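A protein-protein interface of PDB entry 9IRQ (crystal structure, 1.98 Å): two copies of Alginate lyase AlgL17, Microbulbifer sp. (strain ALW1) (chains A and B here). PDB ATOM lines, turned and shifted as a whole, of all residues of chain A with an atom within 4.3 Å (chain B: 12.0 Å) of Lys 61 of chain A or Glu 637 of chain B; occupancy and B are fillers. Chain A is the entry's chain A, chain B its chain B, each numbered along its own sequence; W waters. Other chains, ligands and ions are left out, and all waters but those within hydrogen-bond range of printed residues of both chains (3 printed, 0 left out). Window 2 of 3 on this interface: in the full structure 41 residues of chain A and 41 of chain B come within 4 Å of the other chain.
N of Thr 639 of chain B lies within hydrogen-bond range of OE1 of Glu 58 of chain A (3.0 Å).
The side-chain amino group of Lys 61 of chain A lies within hydrogen-bond range of the backbone carbonyl oxygen of Glu 637 of chain B (2.7 Å).
OE1 of Glu 637 of chain B is in salt-bridge range of NH1 of Arg 233 of chain A (3.0 Å).
The side-chain amino group (NZ) of Lys 289 of chain A lies close to the backbone carbonyl oxygen (O) of Pro 634 of chain B.
The backbone carbonyl oxygen (O) of Ser 635 of chain B lies within hydrogen-bond range of the side-chain amino group (NZ) of Lys 289 of chain A (3.0 Å).
The side-chain amino group (NZ) of Lys 289 of chain A is in salt-bridge range of the side-chain carboxylate (OE1) of Glu 637 of chain B (2.7 Å).
The side-chain hydroxyl (OH) of Tyr 632 of chain B is in hydrogen-bond range of the backbone carbonyl oxygen (O) of Leu 412 of chain A, 2.7 Å away.
The side-chain amide nitrogen (ND2) of Asn 413 of chain A is in hydrogen-bond range of the backbone carbonyl oxygen (O) of Glu 637 of chain B (3.3 Å).
The backbone carbonyl oxygen (O) of Asn 413 of chain A lies within hydrogen-bond range of the side-chain hydroxyl (OG1) of Thr 639 of chain B (2.8 Å).
The side-chain amino group (NZ) of Lys 61 of chain A is in salt-bridge range of the side-chain carboxylate (OE2) of Glu 58 of chain A, at 2.9 Å.
The side-chain amide nitrogen (ND2) of Asn 413 of chain A sits close to the side-chain amino group (NZ) of Lys 61 of chain A, 3.4 Å away.
N of Tyr 632 of chain B lies within hydrogen-bond range of O of Gly 575 of chain B (2.8 Å).
OD1 of Asn 633 of chain B is in hydrogen-bond range of N of Ser 635 of chain B (2.9 Å).
The backbone NH of Asn 633 of chain B sits at hydrogen-bond distance from the backbone carbonyl oxygen of Phe 638 of chain B.
Phe 638 of chain B touches Glu 58 of chain A (CA to OE1, 3.3 Å).
CD2 of Leu 412 of chain A touches CG of Glu 637 of chain B, at 3.98 Å.
Of chain B, only Glu 637 (2.7 Å) comes within 4 Å of Lys 61 of chain A.
Printed residues of chain A within 4 Å of Glu 637 of chain B: Lys 61, Arg 233, Lys 289, Leu 412 and Asn 413.
No residue of chain B comes within 4 Å of Gln 59 of chain A.
No residue of chain B comes within 4 Å of His 60 of chain A.
No residue of chain B comes within 4 Å of Lys 62 of chain A.
No residue of chain B comes within 4 Å of Tyr 64 of chain A.
No residue of chain B comes within 4 Å of Gln 65 of chain A.
Asn 413 of chain A touches just these residues of chain B: Glu 637 (3.3 Å) and Thr 639 (2.8 Å).
Of the printed residues of chain A, Pro 634 of chain B touches Lys 289 (3.4 Å).
Printed residues of chain A within 4 Å of Tyr 632 of chain B: Leu 412 (2.7 Å).
Of the printed residues of chain A, Phe 638 of chain B touches Glu 58.
Printed residues of chain B within 4 Å of Arg 233 of chain A: Glu 637 (3.0 Å).
The nearest printed residue of chain A that does not touch Tyr 632 of chain B is Asn 413 of chain A (4.2 Å).
Printed residues of chain B that touch a printed residue of chain A: Tyr 632, Pro 634, Ser 635, Glu 637, Phe 638 and Thr 639.
Hydrophobic or aromatic side chains of chain B that line the printed part of chain A: Tyr 632 and Phe 638.
Hydrophobic or aromatic side chains of chain A within 4 Å of the printed part of chain B: Leu 412.
No position is printed for both chains.
Of the 11 pairs that touch across the chains among the printed residues, none has its exchanged pair printed and touching as well.
Water W3 bridges the side-chain carboxylate (OE2) of Glu 637 of chain B (2.5 Å) and the guanidinium group (NH2) of Arg 233 of chain A (3.1 Å).
Water W1 bridges OE2 of Glu 637 of chain B (2.7 Å) and ND2 of Asn 413 of chain A (3.0 Å).
Water W2 bridges the backbone NH (N) of Leu 412 of chain A (3.1 Å) and the side-chain hydroxyl (OH) of Tyr 632 of chain B (3.2 Å).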
ATOM      1  N   HIS A  57      -8.527 -27.684 -38.789  1.00  0.00           N
ATOM      2  CA  HIS A  57      -9.272 -28.717 -38.081  1.00  0.00           C
ATOM      3  C   HIS A  57     -10.267 -28.098 -37.100  1.00  0.00           C
ATOM      4  O   HIS A  57     -11.463 -28.413 -37.127  1.00  0.00           O
ATOM      5  CB  HIS A  57      -8.282 -29.634 -37.366  1.00  0.00           C
ATOM      6  CG  HIS A  57      -8.918 -30.759 -36.604  1.00  0.00           C
ATOM      7  ND1 HIS A  57      -9.032 -32.031 -37.122  1.00  0.00           N
ATOM      8  CD2 HIS A  57      -9.458 -30.807 -35.363  1.00  0.00           C
ATOM      9  CE1 HIS A  57      -9.613 -32.816 -36.230  1.00  0.00           C
ATOM     10  NE2 HIS A  57      -9.885 -32.097 -35.155  1.00  0.00           N
ATOM     11  N   GLU A  58      -9.795 -27.197 -36.232  1.00  0.00           N
ATOM     12  CA  GLU A  58     -10.687 -26.607 -35.241  1.00  0.00           C
ATOM     13  C   GLU A  58     -11.641 -25.594 -35.853  1.00  0.00           C
ATOM     14  O   GLU A  58     -12.706 -25.335 -35.275  1.00  0.00           O
ATOM     15  CB  GLU A  58      -9.889 -25.956 -34.110  1.00  0.00           C
ATOM     16  CG  GLU A  58      -9.125 -26.952 -33.249  1.00  0.00           C
ATOM     17  CD  GLU A  58     -10.018 -27.984 -32.554  1.00  0.00           C
ATOM     18  OE1 GLU A  58     -11.068 -27.605 -31.978  1.00  0.00           O
ATOM     19  OE2 GLU A  58      -9.652 -29.181 -32.574  1.00  0.00           O
ATOM     20  N   GLN A  59     -11.295 -25.032 -37.012  1.00  0.00           N
ATOM     21  CA  GLN A  59     -12.202 -24.099 -37.666  1.00  0.00           C
ATOM     22  C   GLN A  59     -13.356 -24.842 -38.315  1.00  0.00           C
ATOM     23  O   GLN A  59     -14.506 -24.405 -38.222  1.00  0.00           O
ATOM     24  CB  GLN A  59     -11.436 -23.260 -38.698  1.00  0.00           C
ATOM     25  CG  GLN A  59     -12.262 -22.232 -39.470  1.00  0.00           C
ATOM     26  CD  GLN A  59     -12.898 -21.195 -38.570  1.00  0.00           C
ATOM     27  OE1 GLN A  59     -12.211 -20.494 -37.838  1.00  0.00           O
ATOM     28  NE2 GLN A  59     -14.219 -21.083 -38.631  1.00  0.00           N
ATOM     29  N   HIS A  60     -13.068 -25.967 -38.985  1.00  0.00           N
ATOM     30  CA  HIS A  60     -14.135 -26.763 -39.593  1.00  0.00           C
ATOM     31  C   HIS A  60     -15.044 -27.377 -38.545  1.00  0.00           C
ATOM     32  O   HIS A  60     -16.245 -27.535 -38.793  1.00  0.00           O
ATOM     33  CB  HIS A  60     -13.535 -27.833 -40.502  1.00  0.00           C
ATOM     34  CG  HIS A  60     -13.070 -27.279 -41.812  1.00  0.00           C
ATOM     35  ND1 HIS A  60     -13.910 -26.584 -42.655  1.00  0.00           N
ATOM     36  CD2 HIS A  60     -11.852 -27.282 -42.410  1.00  0.00           C
ATOM     37  CE1 HIS A  60     -13.234 -26.189 -43.723  1.00  0.00           C
ATOM     38  NE2 HIS A  60     -11.984 -26.604 -43.601  1.00  0.00           N
ATOM     39  N   LYS A  61     -14.498 -27.682 -37.357  1.00  0.00           N
ATOM     40  CA  LYS A  61     -15.328 -28.075 -36.220  1.00  0.00           C
ATOM     41  C   LYS A  61     -16.212 -26.929 -35.748  1.00  0.00           C
ATOM     42  O   LYS A  61     -17.405 -27.123 -35.486  1.00  0.00           O
ATOM     43  CB  LYS A  61     -14.447 -28.544 -35.073  1.00  0.00           C
ATOM     44  CG  LYS A  61     -14.008 -29.968 -35.191  1.00  0.00           C
ATOM     45  CD  LYS A  61     -12.875 -30.237 -34.225  1.00  0.00           C
ATOM     46  CE  LYS A  61     -13.337 -30.170 -32.778  1.00  0.00           C
ATOM     47  NZ  LYS A  61     -12.173 -30.526 -31.924  1.00  0.00           N
ATOM     48  N   LYS A  62     -15.631 -25.728 -35.592  1.00  0.00           N
ATOM     49  CA  LYS A  62     -16.431 -24.563 -35.220  1.00  0.00           C
ATOM     50  C   LYS A  62     -17.562 -24.363 -36.208  1.00  0.00           C
ATOM     51  O   LYS A  62     -18.678 -23.996 -35.825  1.00  0.00           O
ATOM     52  CB  LYS A  62     -15.569 -23.299 -35.194  1.00  0.00           C
ATOM     53  CG  LYS A  62     -15.038 -22.901 -33.837  1.00  0.00           C
ATOM     54  CD  LYS A  62     -14.700 -21.412 -33.825  1.00  0.00           C
ATOM     55  CE  LYS A  62     -15.702 -20.624 -32.974  1.00  0.00           C
ATOM     56  NZ  LYS A  62     -15.796 -21.171 -31.577  1.00  0.00           N
ATOM     57  N   ASN A  63     -17.280 -24.603 -37.487  1.00  0.00           N
ATOM     58  CA  ASN A  63     -18.247 -24.341 -38.544  1.00  0.00           C
ATOM     59  C   ASN A  63     -19.474 -25.237 -38.409  1.00  0.00           C
ATOM     60  O   ASN A  63     -20.613 -24.753 -38.463  1.00  0.00           O
ATOM     61  CB  ASN A  63     -17.581 -24.526 -39.909  1.00  0.00           C
ATOM     62  CG  ASN A  63     -16.688 -23.361 -40.293  1.00  0.00           C
ATOM     63  OD1 ASN A  63     -16.639 -22.349 -39.605  1.00  0.00           O
ATOM     64  ND2 ASN A  63     -15.986 -23.496 -41.408  1.00  0.00           N
ATOM     65  N   TYR A  64     -19.281 -26.551 -38.223  1.00  0.00           N
ATOM     66  CA  TYR A  64     -20.470 -27.402 -38.102  1.00  0.00           C
ATOM     67  C   TYR A  64     -21.248 -27.069 -36.837  1.00  0.00           C
ATOM     68  O   TYR A  64     -22.482 -26.985 -36.865  1.00  0.00           O
ATOM     69  CB  TYR A  64     -20.121 -28.906 -38.204  1.00  0.00           C
ATOM     70  CG  TYR A  64     -19.328 -29.607 -37.097  1.00  0.00           C
ATOM     71  CD1 TYR A  64     -19.859 -29.784 -35.817  1.00  0.00           C
ATOM     72  CD2 TYR A  64     -18.091 -30.201 -37.375  1.00  0.00           C
ATOM     73  CE1 TYR A  64     -19.150 -30.473 -34.825  1.00  0.00           C
ATOM     74  CE2 TYR A  64     -17.384 -30.897 -36.388  1.00  0.00           C
ATOM     75  CZ  TYR A  64     -17.915 -31.027 -35.126  1.00  0.00           C
ATOM     76  OH  TYR A  64     -17.216 -31.693 -34.143  1.00  0.00           O
ATOM     77  N   GLN A  65     -20.552 -26.783 -35.745  1.00  0.00           N
ATOM     78  CA  GLN A  65     -21.254 -26.374 -34.533  1.00  0.00           C
ATOM     79  C   GLN A  65     -22.091 -25.126 -34.792  1.00  0.00           C
ATOM     80  O   GLN A  65     -23.275 -25.072 -34.433  1.00  0.00           O
ATOM     81  CB  GLN A  65     -20.239 -26.149 -33.401  1.00  0.00           C
ATOM     82  CG  GLN A  65     -20.837 -26.034 -32.013  1.00  0.00           C
ATOM     83  CD  GLN A  65     -21.496 -27.318 -31.558  1.00  0.00           C
ATOM     84  OE1 GLN A  65     -22.709 -27.349 -31.325  1.00  0.00           O
ATOM     85  NE2 GLN A  65     -20.709 -28.394 -31.446  1.00  0.00           N
ATOM     86  N   PHE A 117     -10.914 -33.153 -42.937  1.00  0.00           N
ATOM     87  CA  PHE A 117     -10.148 -33.435 -41.740  1.00  0.00           C
ATOM     88  C   PHE A 117      -9.101 -34.496 -42.045  1.00  0.00           C
ATOM     89  O   PHE A 117      -9.198 -35.215 -43.037  1.00  0.00           O
ATOM     90  CB  PHE A 117     -11.076 -33.896 -40.603  1.00  0.00           C
ATOM     91  CG  PHE A 117     -12.160 -32.905 -40.254  1.00  0.00           C
ATOM     92  CD1 PHE A 117     -13.389 -32.946 -40.893  1.00  0.00           C
ATOM     93  CD2 PHE A 117     -11.950 -31.940 -39.268  1.00  0.00           C
ATOM     94  CE1 PHE A 117     -14.390 -32.052 -40.576  1.00  0.00           C
ATOM     95  CE2 PHE A 117     -12.950 -31.037 -38.939  1.00  0.00           C
ATOM     96  CZ  PHE A 117     -14.180 -31.096 -39.592  1.00  0.00           C
ATOM     97  N   ARG A 233     -19.871 -43.097 -24.474  1.00  0.00           N
ATOM     98  CA  ARG A 233     -20.460 -41.776 -24.646  1.00  0.00           C
ATOM     99  C   ARG A 233     -20.174 -41.213 -26.033  1.00  0.00           C
ATOM    100  O   ARG A 233     -21.003 -40.490 -26.576  1.00  0.00           O
ATOM    101  CB  ARG A 233     -19.980 -40.821 -23.558  1.00  0.00           C
ATOM    102  CG  ARG A 233     -18.524 -40.558 -23.564  1.00  0.00           C
ATOM    103  CD  ARG A 233     -18.170 -39.366 -24.470  1.00  0.00           C
ATOM    104  NE  ARG A 233     -16.827 -39.587 -24.969  1.00  0.00           N
ATOM    105  CZ  ARG A 233     -16.157 -38.766 -25.767  1.00  0.00           C
ATOM    106  NH1 ARG A 233     -16.712 -37.644 -26.236  1.00  0.00           N
ATOM    107  NH2 ARG A 233     -14.928 -39.098 -26.113  1.00  0.00           N
ATOM    108  N   LYS A 289     -13.021 -36.385 -19.214  1.00  0.00           N
ATOM    109  CA  LYS A 289     -14.322 -36.467 -19.866  1.00  0.00           C
ATOM    110  C   LYS A 289     -15.393 -36.831 -18.841  1.00  0.00           C
ATOM    111  O   LYS A 289     -15.226 -37.775 -18.066  1.00  0.00           O
ATOM    112  CB  LYS A 289     -14.247 -37.488 -20.999  1.00  0.00           C
ATOM    113  CG  LYS A 289     -15.513 -37.684 -21.845  1.00  0.00           C
ATOM    114  CD  LYS A 289     -16.181 -36.382 -22.283  1.00  0.00           C
ATOM    115  CE  LYS A 289     -15.304 -35.462 -23.104  1.00  0.00           C
ATOM    116  NZ  LYS A 289     -16.099 -34.591 -24.051  1.00  0.00           N
ATOM    117  N   LEU A 412      -5.684 -34.713 -26.196  1.00  0.00           N
ATOM    118  CA  LEU A 412      -6.777 -34.465 -27.116  1.00  0.00           C
ATOM    119  C   LEU A 412      -6.696 -33.068 -27.699  1.00  0.00           C
ATOM    120  O   LEU A 412      -6.585 -32.086 -26.958  1.00  0.00           O
ATOM    121  CB  LEU A 412      -8.090 -34.651 -26.372  1.00  0.00           C
ATOM    122  CG  LEU A 412      -9.334 -34.453 -27.217  1.00  0.00           C
ATOM    123  CD1 LEU A 412      -9.871 -35.816 -27.630  1.00  0.00           C
ATOM    124  CD2 LEU A 412     -10.370 -33.687 -26.402  1.00  0.00           C
ATOM    125  N   ASN A 413      -6.705 -32.993 -29.032  1.00  0.00           N
ATOM    126  CA  ASN A 413      -6.792 -31.723 -29.743  1.00  0.00           C
ATOM    127  C   ASN A 413      -5.665 -30.768 -29.357  1.00  0.00           C
ATOM    128  O   ASN A 413      -5.861 -29.550 -29.339  1.00  0.00           O
ATOM    129  CB  ASN A 413      -8.159 -31.061 -29.519  1.00  0.00           C
ATOM    130  CG  ASN A 413      -9.306 -31.904 -30.052  1.00  0.00           C
ATOM    131  OD1 ASN A 413      -9.165 -32.579 -31.077  1.00  0.00           O
ATOM    132  ND2 ASN A 413     -10.445 -31.883 -29.354  1.00  0.00           N
ATOM    133  N   LEU B 571       0.657 -26.315 -21.085  1.00  0.00           N
ATOM    134  CA  LEU B 571      -0.794 -26.273 -21.004  1.00  0.00           C
ATOM    135  C   LEU B 571      -1.228 -26.482 -19.560  1.00  0.00           C
ATOM    136  O   LEU B 571      -0.811 -27.455 -18.911  1.00  0.00           O
ATOM    137  CB  LEU B 571      -1.417 -27.347 -21.909  1.00  0.00           C
ATOM    138  CG  LEU B 571      -2.913 -27.622 -21.752  1.00  0.00           C
ATOM    139  CD1 LEU B 571      -3.747 -26.380 -22.115  1.00  0.00           C
ATOM    140  CD2 LEU B 571      -3.341 -28.854 -22.569  1.00  0.00           C
ATOM    141  N   GLY B 575      -7.394 -24.590 -18.550  1.00  0.00           N
ATOM    142  CA  GLY B 575      -7.842 -24.387 -19.914  1.00  0.00           C
ATOM    143  C   GLY B 575      -7.019 -23.427 -20.741  1.00  0.00           C
ATOM    144  O   GLY B 575      -7.429 -23.089 -21.865  1.00  0.00           O
ATOM    145  N   PHE B 577      -3.188 -22.119 -22.484  1.00  0.00           N
ATOM    146  CA  PHE B 577      -1.814 -22.354 -22.880  1.00  0.00           C
ATOM    147  C   PHE B 577      -0.977 -21.170 -22.424  1.00  0.00           C
ATOM    148  O   PHE B 577      -1.464 -20.036 -22.341  1.00  0.00           O
ATOM    149  CB  PHE B 577      -1.684 -22.526 -24.397  1.00  0.00           C
ATOM    150  CG  PHE B 577      -2.368 -23.765 -24.942  1.00  0.00           C
ATOM    151  CD1 PHE B 577      -3.724 -23.755 -25.233  1.00  0.00           C
ATOM    152  CD2 PHE B 577      -1.652 -24.929 -25.166  1.00  0.00           C
ATOM    153  CE1 PHE B 577      -4.353 -24.894 -25.735  1.00  0.00           C
ATOM    154  CE2 PHE B 577      -2.275 -26.071 -25.671  1.00  0.00           C
ATOM    155  CZ  PHE B 577      -3.630 -26.043 -25.948  1.00  0.00           C
ATOM    156  N   GLY B 630      -5.075 -18.681 -26.006  1.00  0.00           N
ATOM    157  CA  GLY B 630      -5.889 -19.788 -26.441  1.00  0.00           C
ATOM    158  C   GLY B 630      -6.899 -20.245 -25.415  1.00  0.00           C
ATOM    159  O   GLY B 630      -6.985 -19.755 -24.284  1.00  0.00           O
ATOM    160  N   GLU B 631      -7.702 -21.210 -25.847  1.00  0.00           N
ATOM    161  CA  GLU B 631      -8.626 -21.892 -24.962  1.00  0.00           C
ATOM    162  C   GLU B 631      -8.528 -23.377 -25.242  1.00  0.00           C
ATOM    163  O   GLU B 631      -8.445 -23.802 -26.398  1.00  0.00           O
ATOM    164  CB  GLU B 631     -10.072 -21.397 -25.140  1.00  0.00           C
ATOM    165  CG  GLU B 631     -10.918 -21.405 -23.843  1.00  0.00           C
ATOM    166  CD  GLU B 631     -10.162 -20.867 -22.621  1.00  0.00           C
ATOM    167  OE1 GLU B 631      -9.999 -19.628 -22.524  1.00  0.00           O
ATOM    168  OE2 GLU B 631      -9.746 -21.678 -21.756  1.00  0.00           O
ATOM    169  N   TYR B 632      -8.499 -24.157 -24.180  1.00  0.00           N
ATOM    170  CA  TYR B 632      -8.506 -25.604 -24.291  1.00  0.00           C
ATOM    171  C   TYR B 632      -9.667 -26.092 -23.444  1.00  0.00           C
ATOM    172  O   TYR B 632      -9.678 -25.897 -22.226  1.00  0.00           O
ATOM    173  CB  TYR B 632      -7.176 -26.194 -23.839  1.00  0.00           C
ATOM    174  CG  TYR B 632      -7.127 -27.690 -23.958  1.00  0.00           C
ATOM    175  CD1 TYR B 632      -7.041 -28.295 -25.208  1.00  0.00           C
ATOM    176  CD2 TYR B 632      -7.177 -28.505 -22.820  1.00  0.00           C
ATOM    177  CE1 TYR B 632      -7.009 -29.674 -25.330  1.00  0.00           C
ATOM    178  CE2 TYR B 632      -7.136 -29.886 -22.925  1.00  0.00           C
ATOM    179  CZ  TYR B 632      -7.053 -30.466 -24.194  1.00  0.00           C
ATOM    180  OH  TYR B 632      -7.002 -31.832 -24.348  1.00  0.00           O
ATOM    181  N   ASN B 633     -10.669 -26.670 -24.095  1.00  0.00           N
ATOM    182  CA  ASN B 633     -11.885 -27.106 -23.416  1.00  0.00           C
ATOM    183  C   ASN B 633     -12.054 -28.582 -23.745  1.00  0.00           C
ATOM    184  O   ASN B 633     -12.595 -28.927 -24.812  1.00  0.00           O
ATOM    185  CB  ASN B 633     -13.096 -26.287 -23.853  1.00  0.00           C
ATOM    186  CG  ASN B 633     -14.361 -26.620 -23.066  1.00  0.00           C
ATOM    187  OD1 ASN B 633     -14.579 -27.761 -22.668  1.00  0.00           O
ATOM    188  ND2 ASN B 633     -15.204 -25.617 -22.850  1.00  0.00           N
ATOM    189  N   PRO B 634     -11.606 -29.477 -22.857  1.00  0.00           N
ATOM    190  CA  PRO B 634     -11.736 -30.911 -23.125  1.00  0.00           C
ATOM    191  C   PRO B 634     -13.146 -31.428 -22.893  1.00  0.00           C
ATOM    192  O   PRO B 634     -13.422 -32.592 -23.214  1.00  0.00           O
ATOM    193  CB  PRO B 634     -10.739 -31.531 -22.131  1.00  0.00           C
ATOM    194  CG  PRO B 634     -10.827 -30.605 -20.931  1.00  0.00           C
ATOM    195  CD  PRO B 634     -11.092 -29.208 -21.494  1.00  0.00           C
ATOM    196  N   SER B 635     -14.048 -30.592 -22.369  1.00  0.00           N
ATOM    197  CA  SER B 635     -15.429 -31.007 -22.177  1.00  0.00           C
ATOM    198  C   SER B 635     -16.246 -30.828 -23.461  1.00  0.00           C
ATOM    199  O   SER B 635     -16.925 -31.759 -23.914  1.00  0.00           O
ATOM    200  CB  SER B 635     -16.031 -30.223 -21.010  1.00  0.00           C
ATOM    201  OG  SER B 635     -17.416 -30.016 -21.204  1.00  0.00           O
ATOM    202  N   LYS B 636     -16.185 -29.646 -24.073  1.00  0.00           N
ATOM    203  CA  LYS B 636     -16.791 -29.451 -25.384  1.00  0.00           C
ATOM    204  C   LYS B 636     -15.873 -29.873 -26.521  1.00  0.00           C
ATOM    205  O   LYS B 636     -16.324 -29.943 -27.665  1.00  0.00           O
ATOM    206  CB  LYS B 636     -17.225 -27.987 -25.546  1.00  0.00           C
ATOM    207  CG  LYS B 636     -18.280 -27.600 -24.499  1.00  0.00           C
ATOM    208  CD  LYS B 636     -18.687 -26.131 -24.577  1.00  0.00           C
ATOM    209  CE  LYS B 636     -19.401 -25.685 -23.287  1.00  0.00           C
ATOM    210  NZ  LYS B 636     -18.552 -25.769 -22.040  1.00  0.00           N
ATOM    211  N   GLU B 637     -14.615 -30.183 -26.221  1.00  0.00           N
ATOM    212  CA  GLU B 637     -13.675 -30.799 -27.161  1.00  0.00           C
ATOM    213  C   GLU B 637     -13.321 -29.851 -28.316  1.00  0.00           C
ATOM    214  O   GLU B 637     -13.321 -30.229 -29.494  1.00  0.00           O
ATOM    215  CB  GLU B 637     -14.198 -32.153 -27.665  1.00  0.00           C
ATOM    216  CG  GLU B 637     -14.319 -33.177 -26.513  1.00  0.00           C
ATOM    217  CD  GLU B 637     -14.290 -34.647 -26.950  1.00  0.00           C
ATOM    218  OE1 GLU B 637     -14.639 -35.523 -26.114  1.00  0.00           O
ATOM    219  OE2 GLU B 637     -13.920 -34.937 -28.107  1.00  0.00           O
ATOM    220  N   PHE B 638     -12.984 -28.612 -27.962  1.00  0.00           N
ATOM    221  CA  PHE B 638     -12.399 -27.670 -28.905  1.00  0.00           C
ATOM    222  C   PHE B 638     -11.119 -27.093 -28.317  1.00  0.00           C
ATOM    223  O   PHE B 638     -10.911 -27.091 -27.096  1.00  0.00           O
ATOM    224  CB  PHE B 638     -13.379 -26.539 -29.294  1.00  0.00           C
ATOM    225  CG  PHE B 638     -13.661 -25.545 -28.188  1.00  0.00           C
ATOM    226  CD1 PHE B 638     -12.849 -24.430 -28.008  1.00  0.00           C
ATOM    227  CD2 PHE B 638     -14.761 -25.706 -27.355  1.00  0.00           C
ATOM    228  CE1 PHE B 638     -13.115 -23.509 -26.988  1.00  0.00           C
ATOM    229  CE2 PHE B 638     -15.042 -24.792 -26.346  1.00  0.00           C
ATOM    230  CZ  PHE B 638     -14.218 -23.692 -26.160  1.00  0.00           C
ATOM    231  N   THR B 639     -10.262 -26.608 -29.219  1.00  0.00           N
ATOM    232  CA  THR B 639      -9.019 -25.927 -28.885  1.00  0.00           C
ATOM    233  C   THR B 639      -8.894 -24.716 -29.788  1.00  0.00           C
ATOM    234  O   THR B 639      -9.134 -24.809 -30.994  1.00  0.00           O
ATOM    235  CB  THR B 639      -7.795 -26.819 -29.096  1.00  0.00           C
ATOM    236  OG1 THR B 639      -7.933 -28.019 -28.322  1.00  0.00           O
ATOM    237  CG2 THR B 639      -6.527 -26.089 -28.693  1.00  0.00           C
ATOM    238  N   LEU B 640      -8.523 -23.586 -29.211  1.00  0.00           N
ATOM    239  CA  LEU B 640      -8.329 -22.372 -29.986  1.00  0.00           C
ATOM    240  C   LEU B 640      -6.965 -21.788 -29.652  1.00  0.00           C
ATOM    241  O   LEU B 640      -6.545 -21.804 -28.492  1.00  0.00           O
ATOM    242  CB  LEU B 640      -9.440 -21.347 -29.705  1.00  0.00           C
ATOM    243  CG  LEU B 640      -9.427 -20.022 -30.483  1.00  0.00           C
ATOM    244  CD1 LEU B 640      -9.132 -20.206 -31.981  1.00  0.00           C
ATOM    245  CD2 LEU B 640     -10.745 -19.296 -30.290  1.00  0.00           C
ATOM    246  N   GLU B 641      -6.263 -21.330 -30.687  1.00  0.00           N
ATOM    247  CA  GLU B 641      -5.022 -20.576 -30.548  1.00  0.00           C
ATOM    248  C   GLU B 641      -4.023 -21.277 -29.630  1.00  0.00           C
ATOM    249  O   GLU B 641      -3.400 -20.666 -28.760  1.00  0.00           O
ATOM    250  CB  GLU B 641      -5.321 -19.159 -30.066  1.00  0.00           C
ATOM    251  CG  GLU B 641      -6.087 -18.352 -31.116  1.00  0.00           C
ATOM    252  CD  GLU B 641      -6.363 -16.924 -30.680  1.00  0.00           C
ATOM    253  OE1 GLU B 641      -6.851 -16.132 -31.523  1.00  0.00           O
ATOM    254  OE2 GLU B 641      -6.093 -16.595 -29.499  1.00  0.00           O
ATOM    255  N   ALA B 642      -3.871 -22.585 -29.833  1.00  0.00           N
ATOM    256  CA  ALA B 642      -2.921 -23.337 -29.026  1.00  0.00           C
ATOM    257  C   ALA B 642      -1.489 -22.916 -29.300  1.00  0.00           C
ATOM    258  O   ALA B 642      -0.613 -23.111 -28.448  1.00  0.00           O
ATOM    259  CB  ALA B 642      -3.059 -24.834 -29.290  1.00  0.00           C
HETATM  260  O   HOH W   1     -12.548 -33.933 -30.175  1.00  0.00           O
HETATM  261  O   HOH W   2      -6.182 -34.678 -23.154  1.00  0.00           O
HETATM  262  O   HOH W   3     -13.545 -37.379 -28.297  1.00  0.00           O
